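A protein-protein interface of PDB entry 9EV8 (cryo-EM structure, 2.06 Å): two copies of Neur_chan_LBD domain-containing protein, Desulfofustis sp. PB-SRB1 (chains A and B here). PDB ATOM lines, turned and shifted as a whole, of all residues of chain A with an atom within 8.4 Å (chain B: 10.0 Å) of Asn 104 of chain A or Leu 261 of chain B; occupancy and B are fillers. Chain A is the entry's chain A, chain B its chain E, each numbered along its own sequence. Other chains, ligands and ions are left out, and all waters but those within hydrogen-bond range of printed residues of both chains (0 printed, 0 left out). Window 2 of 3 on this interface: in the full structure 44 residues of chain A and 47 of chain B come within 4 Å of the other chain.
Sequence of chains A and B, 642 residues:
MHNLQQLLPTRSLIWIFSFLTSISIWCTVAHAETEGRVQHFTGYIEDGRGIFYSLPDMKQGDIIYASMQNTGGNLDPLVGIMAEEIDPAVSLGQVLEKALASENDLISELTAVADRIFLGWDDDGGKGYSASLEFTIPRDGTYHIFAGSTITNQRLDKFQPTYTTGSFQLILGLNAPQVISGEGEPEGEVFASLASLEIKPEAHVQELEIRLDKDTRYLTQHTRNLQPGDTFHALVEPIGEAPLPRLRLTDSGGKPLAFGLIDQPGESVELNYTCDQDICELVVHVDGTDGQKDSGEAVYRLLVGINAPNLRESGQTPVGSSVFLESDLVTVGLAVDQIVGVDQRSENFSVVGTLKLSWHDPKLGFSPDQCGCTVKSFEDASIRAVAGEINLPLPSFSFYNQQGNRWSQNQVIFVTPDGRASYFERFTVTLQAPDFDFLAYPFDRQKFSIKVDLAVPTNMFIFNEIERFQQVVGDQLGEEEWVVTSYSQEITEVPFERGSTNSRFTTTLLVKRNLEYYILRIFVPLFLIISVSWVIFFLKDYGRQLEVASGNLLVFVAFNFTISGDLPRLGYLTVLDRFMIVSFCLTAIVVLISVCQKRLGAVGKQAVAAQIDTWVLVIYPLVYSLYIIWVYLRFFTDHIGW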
ATOM      1  N   VAL A  95     -18.857 -21.034  14.290  1.00  0.00           N
ATOM      2  CA  VAL A  95     -17.755 -21.916  14.659  1.00  0.00           C
ATOM      3  C   VAL A  95     -16.660 -21.864  13.601  1.00  0.00           C
ATOM      4  O   VAL A  95     -15.469 -21.803  13.925  1.00  0.00           O
ATOM      5  CB  VAL A  95     -18.269 -23.349  14.878  1.00  0.00           C
ATOM      6  CG1 VAL A  95     -17.127 -24.272  15.268  1.00  0.00           C
ATOM      7  CG2 VAL A  95     -19.354 -23.360  15.940  1.00  0.00           C
ATOM      8  N   LYS A  98     -14.616 -18.646  13.840  1.00  0.00           N
ATOM      9  CA  LYS A  98     -13.618 -18.548  14.908  1.00  0.00           C
ATOM     10  C   LYS A  98     -12.415 -19.428  14.571  1.00  0.00           C
ATOM     11  O   LYS A  98     -11.912 -20.200  15.388  1.00  0.00           O
ATOM     12  CB  LYS A  98     -14.227 -18.949  16.244  1.00  0.00           C
ATOM     13  CG  LYS A  98     -15.372 -18.080  16.730  1.00  0.00           C
ATOM     14  CD  LYS A  98     -16.077 -18.737  17.911  1.00  0.00           C
ATOM     15  CE  LYS A  98     -17.030 -17.777  18.603  1.00  0.00           C
ATOM     16  NZ  LYS A  98     -16.294 -16.680  19.291  1.00  0.00           N
ATOM     17  N   ASN A 104      -8.594 -25.230  22.589  1.00  0.00           N
ATOM     18  CA  ASN A 104      -9.330 -26.238  21.835  1.00  0.00           C
ATOM     19  C   ASN A 104     -10.243 -25.547  20.831  1.00  0.00           C
ATOM     20  O   ASN A 104     -11.470 -25.645  20.923  1.00  0.00           O
ATOM     21  CB  ASN A 104     -10.128 -27.152  22.769  1.00  0.00           C
ATOM     22  CG  ASN A 104      -9.258 -27.823  23.816  1.00  0.00           C
ATOM     23  OD1 ASN A 104      -8.060 -28.019  23.610  1.00  0.00           O
ATOM     24  ND2 ASN A 104      -9.861 -28.177  24.946  1.00  0.00           N
ATOM     25  N   ASP A 105      -9.641 -24.852  19.864  1.00  0.00           N
ATOM     26  CA  ASP A 105     -10.343 -23.889  19.029  1.00  0.00           C
ATOM     27  C   ASP A 105     -11.434 -24.515  18.165  1.00  0.00           C
ATOM     28  O   ASP A 105     -12.326 -23.806  17.687  1.00  0.00           O
ATOM     29  CB  ASP A 105      -9.331 -23.147  18.147  1.00  0.00           C
ATOM     30  CG  ASP A 105      -9.983 -22.111  17.248  1.00  0.00           C
ATOM     31  OD1 ASP A 105     -10.757 -21.281  17.761  1.00  0.00           O
ATOM     32  OD2 ASP A 105      -9.709 -22.124  16.028  1.00  0.00           O
ATOM     33  N   LEU A 106     -11.401 -25.833  17.973  1.00  0.00           N
ATOM     34  CA  LEU A 106     -12.399 -26.457  17.114  1.00  0.00           C
ATOM     35  C   LEU A 106     -13.290 -27.435  17.866  1.00  0.00           C
ATOM     36  O   LEU A 106     -14.519 -27.309  17.833  1.00  0.00           O
ATOM     37  CB  LEU A 106     -11.723 -27.170  15.944  1.00  0.00           C
ATOM     38  CG  LEU A 106     -12.678 -27.705  14.876  1.00  0.00           C
ATOM     39  CD1 LEU A 106     -13.482 -26.565  14.272  1.00  0.00           C
ATOM     40  CD2 LEU A 106     -11.920 -28.457  13.795  1.00  0.00           C
ATOM     41  N   ILE A 107     -12.685 -28.410  18.552  1.00  0.00           N
ATOM     42  CA  ILE A 107     -13.469 -29.486  19.154  1.00  0.00           C
ATOM     43  C   ILE A 107     -14.328 -28.968  20.299  1.00  0.00           C
ATOM     44  O   ILE A 107     -15.524 -29.280  20.374  1.00  0.00           O
ATOM     45  CB  ILE A 107     -12.538 -30.623  19.615  1.00  0.00           C
ATOM     46  CG1 ILE A 107     -11.874 -31.285  18.408  1.00  0.00           C
ATOM     47  CG2 ILE A 107     -13.305 -31.651  20.428  1.00  0.00           C
ATOM     48  CD1 ILE A 107     -10.940 -32.417  18.772  1.00  0.00           C
ATOM     49  N   SER A 108     -13.752 -28.165  21.196  1.00  0.00           N
ATOM     50  CA  SER A 108     -14.521 -27.646  22.322  1.00  0.00           C
ATOM     51  C   SER A 108     -15.649 -26.739  21.847  1.00  0.00           C
ATOM     52  O   SER A 108     -16.772 -26.811  22.356  1.00  0.00           O
ATOM     53  CB  SER A 108     -13.603 -26.899  23.289  1.00  0.00           C
ATOM     54  OG  SER A 108     -14.332 -26.390  24.394  1.00  0.00           O
ATOM     55  N   GLU A 109     -15.361 -25.867  20.880  1.00  0.00           N
ATOM     56  CA  GLU A 109     -16.390 -24.967  20.370  1.00  0.00           C
ATOM     57  C   GLU A 109     -17.521 -25.739  19.703  1.00  0.00           C
ATOM     58  O   GLU A 109     -18.703 -25.443  19.928  1.00  0.00           O
ATOM     59  CB  GLU A 109     -15.771 -23.965  19.396  1.00  0.00           C
ATOM     60  CG  GLU A 109     -14.625 -23.154  19.982  1.00  0.00           C
ATOM     61  CD  GLU A 109     -15.078 -22.179  21.053  1.00  0.00           C
ATOM     62  OE1 GLU A 109     -16.281 -21.849  21.092  1.00  0.00           O
ATOM     63  OE2 GLU A 109     -14.228 -21.740  21.858  1.00  0.00           O
ATOM     64  N   LEU A 110     -17.181 -26.744  18.891  1.00  0.00           N
ATOM     65  CA  LEU A 110     -18.214 -27.544  18.249  1.00  0.00           C
ATOM     66  C   LEU A 110     -19.052 -28.287  19.277  1.00  0.00           C
ATOM     67  O   LEU A 110     -20.279 -28.352  19.155  1.00  0.00           O
ATOM     68  CB  LEU A 110     -17.586 -28.521  17.256  1.00  0.00           C
ATOM     69  CG  LEU A 110     -18.552 -29.443  16.512  1.00  0.00           C
ATOM     70  CD1 LEU A 110     -19.529 -28.636  15.680  1.00  0.00           C
ATOM     71  CD2 LEU A 110     -17.788 -30.421  15.640  1.00  0.00           C
ATOM     72  N   THR A 111     -18.410 -28.848  20.306  1.00  0.00           N
ATOM     73  CA  THR A 111     -19.156 -29.564  21.335  1.00  0.00           C
ATOM     74  C   THR A 111     -20.083 -28.626  22.096  1.00  0.00           C
ATOM     75  O   THR A 111     -21.245 -28.962  22.358  1.00  0.00           O
ATOM     76  CB  THR A 111     -18.189 -30.261  22.294  1.00  0.00           C
ATOM     77  OG1 THR A 111     -17.313 -31.120  21.554  1.00  0.00           O
ATOM     78  CG2 THR A 111     -18.949 -31.091  23.313  1.00  0.00           C
ATOM     79  N   PHE A 159      -3.491 -26.248   8.435  1.00  0.00           N
ATOM     80  CA  PHE A 159      -4.746 -26.471   9.140  1.00  0.00           C
ATOM     81  C   PHE A 159      -5.811 -25.541   8.573  1.00  0.00           C
ATOM     82  O   PHE A 159      -5.635 -24.318   8.571  1.00  0.00           O
ATOM     83  CB  PHE A 159      -4.566 -26.245  10.640  1.00  0.00           C
ATOM     84  CG  PHE A 159      -5.765 -26.623  11.459  1.00  0.00           C
ATOM     85  CD1 PHE A 159      -5.979 -27.935  11.830  1.00  0.00           C
ATOM     86  CD2 PHE A 159      -6.672 -25.661  11.867  1.00  0.00           C
ATOM     87  CE1 PHE A 159      -7.081 -28.285  12.584  1.00  0.00           C
ATOM     88  CE2 PHE A 159      -7.772 -26.003  12.623  1.00  0.00           C
ATOM     89  CZ  PHE A 159      -7.978 -27.318  12.982  1.00  0.00           C
ATOM     90  N   ALA B 234       2.139 -34.419  24.789  1.00  0.00           N
ATOM     91  CA  ALA B 234       3.113 -33.632  24.049  1.00  0.00           C
ATOM     92  C   ALA B 234       3.199 -32.237  24.653  1.00  0.00           C
ATOM     93  O   ALA B 234       2.217 -31.720  25.194  1.00  0.00           O
ATOM     94  CB  ALA B 234       2.754 -33.542  22.562  1.00  0.00           C
ATOM     95  N   LEU B 235       4.380 -31.632  24.551  1.00  0.00           N
ATOM     96  CA  LEU B 235       4.594 -30.276  25.033  1.00  0.00           C
ATOM     97  C   LEU B 235       5.718 -29.630  24.234  1.00  0.00           C
ATOM     98  O   LEU B 235       6.587 -30.317  23.694  1.00  0.00           O
ATOM     99  CB  LEU B 235       4.915 -30.251  26.534  1.00  0.00           C
ATOM    100  CG  LEU B 235       6.143 -31.015  27.038  1.00  0.00           C
ATOM    101  CD1 LEU B 235       7.365 -30.109  27.122  1.00  0.00           C
ATOM    102  CD2 LEU B 235       5.852 -31.650  28.388  1.00  0.00           C
ATOM    103  N   VAL B 236       5.693 -28.301  24.168  1.00  0.00           N
ATOM    104  CA  VAL B 236       6.675 -27.526  23.420  1.00  0.00           C
ATOM    105  C   VAL B 236       7.173 -26.381  24.293  1.00  0.00           C
ATOM    106  O   VAL B 236       6.381 -25.697  24.950  1.00  0.00           O
ATOM    107  CB  VAL B 236       6.088 -27.000  22.094  1.00  0.00           C
ATOM    108  CG1 VAL B 236       4.778 -26.268  22.337  1.00  0.00           C
ATOM    109  CG2 VAL B 236       7.082 -26.101  21.381  1.00  0.00           C
ATOM    110  N   LEU B 244       5.697 -18.234  21.270  1.00  0.00           N
ATOM    111  CA  LEU B 244       5.069 -19.543  21.416  1.00  0.00           C
ATOM    112  C   LEU B 244       4.259 -19.883  20.169  1.00  0.00           C
ATOM    113  O   LEU B 244       3.367 -19.115  19.785  1.00  0.00           O
ATOM    114  CB  LEU B 244       4.170 -19.569  22.650  1.00  0.00           C
ATOM    115  CG  LEU B 244       4.874 -19.485  24.004  1.00  0.00           C
ATOM    116  CD1 LEU B 244       3.862 -19.473  25.140  1.00  0.00           C
ATOM    117  CD2 LEU B 244       5.847 -20.643  24.166  1.00  0.00           C
ATOM    118  N   PRO B 245       4.527 -21.012  19.522  1.00  0.00           N
ATOM    119  CA  PRO B 245       3.743 -21.408  18.351  1.00  0.00           C
ATOM    120  C   PRO B 245       2.485 -22.167  18.755  1.00  0.00           C
ATOM    121  O   PRO B 245       2.282 -22.525  19.915  1.00  0.00           O
ATOM    122  CB  PRO B 245       4.711 -22.311  17.584  1.00  0.00           C
ATOM    123  CG  PRO B 245       5.523 -22.950  18.662  1.00  0.00           C
ATOM    124  CD  PRO B 245       5.652 -21.928  19.769  1.00  0.00           C
ATOM    125  N   ARG B 246       1.636 -22.414  17.761  1.00  0.00           N
ATOM    126  CA  ARG B 246       0.414 -23.178  17.976  1.00  0.00           C
ATOM    127  C   ARG B 246       0.675 -24.666  17.779  1.00  0.00           C
ATOM    128  O   ARG B 246       1.495 -25.062  16.946  1.00  0.00           O
ATOM    129  CB  ARG B 246      -0.683 -22.706  17.028  1.00  0.00           C
ATOM    130  CG  ARG B 246      -0.867 -21.202  16.995  1.00  0.00           C
ATOM    131  CD  ARG B 246      -2.035 -20.806  16.111  1.00  0.00           C
ATOM    132  NE  ARG B 246      -3.311 -21.152  16.724  1.00  0.00           N
ATOM    133  CZ  ARG B 246      -3.983 -20.354  17.544  1.00  0.00           C
ATOM    134  NH1 ARG B 246      -3.531 -19.154  17.864  1.00  0.00           N
ATOM    135  NH2 ARG B 246      -5.138 -20.774  18.055  1.00  0.00           N
ATOM    136  N   LEU B 247      -0.026 -25.489  18.554  1.00  0.00           N
ATOM    137  CA  LEU B 247       0.154 -26.936  18.542  1.00  0.00           C
ATOM    138  C   LEU B 247      -1.207 -27.613  18.468  1.00  0.00           C
ATOM    139  O   LEU B 247      -2.149 -27.185  19.141  1.00  0.00           O
ATOM    140  CB  LEU B 247       0.909 -27.397  19.792  1.00  0.00           C
ATOM    141  CG  LEU B 247       1.321 -28.864  19.889  1.00  0.00           C
ATOM    142  CD1 LEU B 247       2.490 -29.158  18.965  1.00  0.00           C
ATOM    143  CD2 LEU B 247       1.664 -29.222  21.319  1.00  0.00           C
ATOM    144  N   ARG B 248      -1.311 -28.662  17.652  1.00  0.00           N
ATOM    145  CA  ARG B 248      -2.560 -29.399  17.515  1.00  0.00           C
ATOM    146  C   ARG B 248      -2.266 -30.825  17.072  1.00  0.00           C
ATOM    147  O   ARG B 248      -1.179 -31.133  16.581  1.00  0.00           O
ATOM    148  CB  ARG B 248      -3.515 -28.712  16.529  1.00  0.00           C
ATOM    149  CG  ARG B 248      -3.024 -28.680  15.098  1.00  0.00           C
ATOM    150  CD  ARG B 248      -4.023 -27.985  14.186  1.00  0.00           C
ATOM    151  NE  ARG B 248      -4.066 -26.547  14.413  1.00  0.00           N
ATOM    152  CZ  ARG B 248      -3.332 -25.661  13.749  1.00  0.00           C
ATOM    153  NH1 ARG B 248      -2.481 -26.037  12.811  1.00  0.00           N
ATOM    154  NH2 ARG B 248      -3.457 -24.370  14.039  1.00  0.00           N
ATOM    155  N   LEU B 249      -3.256 -31.699  17.258  1.00  0.00           N
ATOM    156  CA  LEU B 249      -3.132 -33.118  16.949  1.00  0.00           C
ATOM    157  C   LEU B 249      -4.271 -33.544  16.036  1.00  0.00           C
ATOM    158  O   LEU B 249      -5.439 -33.264  16.326  1.00  0.00           O
ATOM    159  CB  LEU B 249      -3.144 -33.960  18.230  1.00  0.00           C
ATOM    160  CG  LEU B 249      -2.984 -35.473  18.075  1.00  0.00           C
ATOM    161  CD1 LEU B 249      -1.547 -35.892  18.345  1.00  0.00           C
ATOM    162  CD2 LEU B 249      -3.942 -36.216  18.988  1.00  0.00           C
ATOM    163  N   PRO B 256      -9.337 -33.237  13.315  1.00  0.00           N
ATOM    164  CA  PRO B 256      -8.766 -32.784  14.588  1.00  0.00           C
ATOM    165  C   PRO B 256      -9.211 -33.659  15.750  1.00  0.00           C
ATOM    166  O   PRO B 256     -10.331 -34.174  15.773  1.00  0.00           O
ATOM    167  CB  PRO B 256      -9.299 -31.353  14.727  1.00  0.00           C
ATOM    168  CG  PRO B 256     -10.523 -31.323  13.889  1.00  0.00           C
ATOM    169  CD  PRO B 256     -10.272 -32.254  12.744  1.00  0.00           C
ATOM    170  N   LEU B 257      -8.316 -33.826  16.717  1.00  0.00           N
ATOM    171  CA  LEU B 257      -8.570 -34.627  17.908  1.00  0.00           C
ATOM    172  C   LEU B 257      -8.297 -33.877  19.202  1.00  0.00           C
ATOM    173  O   LEU B 257      -9.019 -34.076  20.181  1.00  0.00           O
ATOM    174  CB  LEU B 257      -7.729 -35.911  17.865  1.00  0.00           C
ATOM    175  CG  LEU B 257      -8.023 -36.877  16.719  1.00  0.00           C
ATOM    176  CD1 LEU B 257      -7.062 -38.050  16.748  1.00  0.00           C
ATOM    177  CD2 LEU B 257      -9.459 -37.361  16.784  1.00  0.00           C
ATOM    178  N   ALA B 258      -7.276 -33.022  19.234  1.00  0.00           N
ATOM    179  CA  ALA B 258      -6.959 -32.247  20.423  1.00  0.00           C
ATOM    180  C   ALA B 258      -6.257 -30.963  20.009  1.00  0.00           C
ATOM    181  O   ALA B 258      -5.704 -30.862  18.911  1.00  0.00           O
ATOM    182  CB  ALA B 258      -6.090 -33.046  21.401  1.00  0.00           C
ATOM    183  N   PHE B 259      -6.284 -29.979  20.904  1.00  0.00           N
ATOM    184  CA  PHE B 259      -5.664 -28.682  20.668  1.00  0.00           C
ATOM    185  C   PHE B 259      -4.837 -28.287  21.881  1.00  0.00           C
ATOM    186  O   PHE B 259      -5.162 -28.660  23.013  1.00  0.00           O
ATOM    187  CB  PHE B 259      -6.713 -27.609  20.364  1.00  0.00           C
ATOM    188  CG  PHE B 259      -6.128 -26.284  19.976  1.00  0.00           C
ATOM    189  CD1 PHE B 259      -5.611 -26.084  18.706  1.00  0.00           C
ATOM    190  CD2 PHE B 259      -6.093 -25.235  20.881  1.00  0.00           C
ATOM    191  CE1 PHE B 259      -5.068 -24.865  18.347  1.00  0.00           C
ATOM    192  CE2 PHE B 259      -5.551 -24.014  20.526  1.00  0.00           C
ATOM    193  CZ  PHE B 259      -5.037 -23.829  19.259  1.00  0.00           C
ATOM    194  N   GLY B 260      -3.766 -27.536  21.642  1.00  0.00           N
ATOM    195  CA  GLY B 260      -2.833 -27.215  22.711  1.00  0.00           C
ATOM    196  C   GLY B 260      -3.348 -26.106  23.610  1.00  0.00           C
ATOM    197  O   GLY B 260      -3.989 -25.154  23.164  1.00  0.00           O
ATOM    198  N   LEU B 261      -3.052 -26.231  24.903  1.00  0.00           N
ATOM    199  CA  LEU B 261      -3.447 -25.258  25.909  1.00  0.00           C
ATOM    200  C   LEU B 261      -2.212 -24.553  26.451  1.00  0.00           C
ATOM    201  O   LEU B 261      -1.237 -25.207  26.833  1.00  0.00           O
ATOM    202  CB  LEU B 261      -4.210 -25.930  27.055  1.00  0.00           C
ATOM    203  CG  LEU B 261      -5.339 -26.886  26.662  1.00  0.00           C
ATOM    204  CD1 LEU B 261      -6.078 -27.372  27.900  1.00  0.00           C
ATOM    205  CD2 LEU B 261      -6.297 -26.231  25.682  1.00  0.00           C
ATOM    206  N   VAL B 269       3.251 -24.942  25.820  1.00  0.00           N
ATOM    207  CA  VAL B 269       1.940 -25.408  25.385  1.00  0.00           C
ATOM    208  C   VAL B 269       1.916 -26.927  25.486  1.00  0.00           C
ATOM    209  O   VAL B 269       2.898 -27.591  25.141  1.00  0.00           O
ATOM    210  CB  VAL B 269       1.617 -24.947  23.947  1.00  0.00           C
ATOM    211  CG1 VAL B 269       0.200 -25.336  23.567  1.00  0.00           C
ATOM    212  CG2 VAL B 269       1.814 -23.447  23.813  1.00  0.00           C
ATOM    213  N   GLU B 270       0.796 -27.477  25.950  1.00  0.00           N
ATOM    214  CA  GLU B 270       0.687 -28.906  26.205  1.00  0.00           C
ATOM    215  C   GLU B 270      -0.605 -29.445  25.604  1.00  0.00           C
ATOM    216  O   GLU B 270      -1.554 -28.701  25.348  1.00  0.00           O
ATOM    217  CB  GLU B 270       0.743 -29.212  27.709  1.00  0.00           C
ATOM    218  CG  GLU B 270      -0.327 -28.508  28.528  1.00  0.00           C
ATOM    219  CD  GLU B 270      -0.174 -28.749  30.019  1.00  0.00           C
ATOM    220  OE1 GLU B 270       0.859 -29.321  30.428  1.00  0.00           O
ATOM    221  OE2 GLU B 270      -1.085 -28.365  30.781  1.00  0.00           O
ATOM    222  N   LEU B 271      -0.628 -30.759  25.385  1.00  0.00           N
ATOM    223  CA  LEU B 271      -1.732 -31.429  24.714  1.00  0.00           C
ATOM    224  C   LEU B 271      -1.887 -32.830  25.290  1.00  0.00           C
ATOM    225  O   LEU B 271      -0.921 -33.419  25.783  1.00  0.00           O
ATOM    226  CB  LEU B 271      -1.492 -31.474  23.197  1.00  0.00           C
ATOM    227  CG  LEU B 271      -2.489 -32.130  22.242  1.00  0.00           C
ATOM    228  CD1 LEU B 271      -2.489 -31.387  20.921  1.00  0.00           C
ATOM    229  CD2 LEU B 271      -2.141 -33.592  22.014  1.00  0.00           C
ATOM    230  N   ASN B 272      -3.107 -33.361  25.228  1.00  0.00           N
ATOM    231  CA  ASN B 272      -3.410 -34.675  25.779  1.00  0.00           C
ATOM    232  C   ASN B 272      -4.502 -35.346  24.959  1.00  0.00           C
ATOM    233  O   ASN B 272      -5.392 -34.674  24.433  1.00  0.00           O
ATOM    234  CB  ASN B 272      -3.841 -34.568  27.247  1.00  0.00           C
ATOM    235  CG  ASN B 272      -4.041 -35.924  27.900  1.00  0.00           C
ATOM    236  OD1 ASN B 272      -3.553 -36.943  27.411  1.00  0.00           O
ATOM    237  ND2 ASN B 272      -4.758 -35.937  29.018  1.00  0.00           N
ATOM    238  N   TYR B 273      -4.432 -36.672  24.856  1.00  0.00           N
ATOM    239  CA  TYR B 273      -5.415 -37.436  24.103  1.00  0.00           C
ATOM    240  C   TYR B 273      -5.445 -38.867  24.623  1.00  0.00           C
ATOM    241  O   TYR B 273      -4.497 -39.339  25.252  1.00  0.00           O
ATOM    242  CB  TYR B 273      -5.108 -37.402  22.598  1.00  0.00           C
ATOM    243  CG  TYR B 273      -6.070 -38.199  21.748  1.00  0.00           C
ATOM    244  CD1 TYR B 273      -7.365 -37.758  21.534  1.00  0.00           C
ATOM    245  CD2 TYR B 273      -5.682 -39.397  21.167  1.00  0.00           C
ATOM    246  CE1 TYR B 273      -8.248 -38.484  20.764  1.00  0.00           C
ATOM    247  CE2 TYR B 273      -6.558 -40.129  20.395  1.00  0.00           C
ATOM    248  CZ  TYR B 273      -7.840 -39.667  20.197  1.00  0.00           C
ATOM    249  OH  TYR B 273      -8.718 -40.394  19.426  1.00  0.00           O
ATOM    250  N   ARG B 312       6.346 -33.534  32.232  1.00  0.00           N
ATOM    251  CA  ARG B 312       6.768 -32.282  32.852  1.00  0.00           C
ATOM    252  C   ARG B 312       8.123 -32.437  33.530  1.00  0.00           C
ATOM    253  O   ARG B 312       9.013 -31.594  33.361  1.00  0.00           O
ATOM    254  CB  ARG B 312       5.718 -31.810  33.860  1.00  0.00           C
ATOM    255  CG  ARG B 312       4.354 -31.528  33.255  1.00  0.00           C
ATOM    256  CD  ARG B 312       3.371 -31.038  34.309  1.00  0.00           C
ATOM    257  NE  ARG B 312       2.060 -30.756  33.739  1.00  0.00           N
ATOM    258  CZ  ARG B 312       1.015 -30.331  34.437  1.00  0.00           C
ATOM    259  NH1 ARG B 312       1.090 -30.127  35.741  1.00  0.00           N
ATOM    260  NH2 ARG B 312      -0.137 -30.106  33.809  1.00  0.00           N
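The backbone carbonyl oxygen (O) of Phe 259 of chain B sits close to the side-chain amide oxygen (OD1) of Asn 104 of chain A, 3.0 Å away.
O of Ile 107 of chain A sits at hydrogen-bond distance from OG1 of Thr 111 of chain A (2.8 Å).
The backbone carbonyl oxygen of Leu 249 of chain B sits at hydrogen-bond distance from the backbone NH of Leu 257 of chain B (3.0 Å).
The backbone NH (N) of Leu 249 of chain B sits at hydrogen-bond distance from the backbone carbonyl oxygen (O) of Ala 258 of chain B (3.1 Å).
The backbone NH of Leu 261 of chain B is in hydrogen-bond range of the backbone carbonyl oxygen of Glu 270 of chain B (2.9 Å).
Among the printed residues, pairs that only touch across the chains: Ile 107 of chain A with Leu 257 of chain B (2.9 Å), Phe 159 of chain A with Arg 248 of chain B (3.0 Å), Leu 106 of chain A with Pro 256 of chain B (3.2 Å), Asn 104 of chain A with Leu 261 of chain B (3.3 Å), Ile 107 of chain A with Pro 256 of chain B (3.5 Å), Asp 105 of chain A with Phe 259 of chain B (3.7 Å) and Ile 107 of chain A with Ala 258 of chain B (3.7 Å).
Asn 104 of chain A touches two residues of chain B.
Leu 261 of chain B touches just one residue of chain A: Asn 104.
No residue of chain B comes within 4 Å of Ser 108 of chain A.
No residue of chain A comes within 4 Å of Gly 260 of chain B.
Of the printed residues of chain A, Ala 258 of chain B touches Ile 107 (3.7 Å).
Of the printed residues of chain B, Phe 159 of chain A touches Arg 248.
Of the printed residues of chain A, Arg 248 of chain B touches Phe 159.
Glu 109 of chain A touches none of the printed residues of chain B.
Leu 271 of chain B touches none of the printed residues of chain A.
Printed residues of chain A that touch a printed residue of chain B: Asn 104, Asp 105, Leu 106, Ile 107 and Phe 159.
Hydrophobic or aromatic side chains of chain B within 4 Å of the printed part of chain A: Pro 256, Phe 259 and Leu 261.
Among the printed residues, no Asp or Glu carboxylate lies within 4 Å of a Lys or Arg side-chain nitrogen of the other chain.
No position is printed for both chains.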
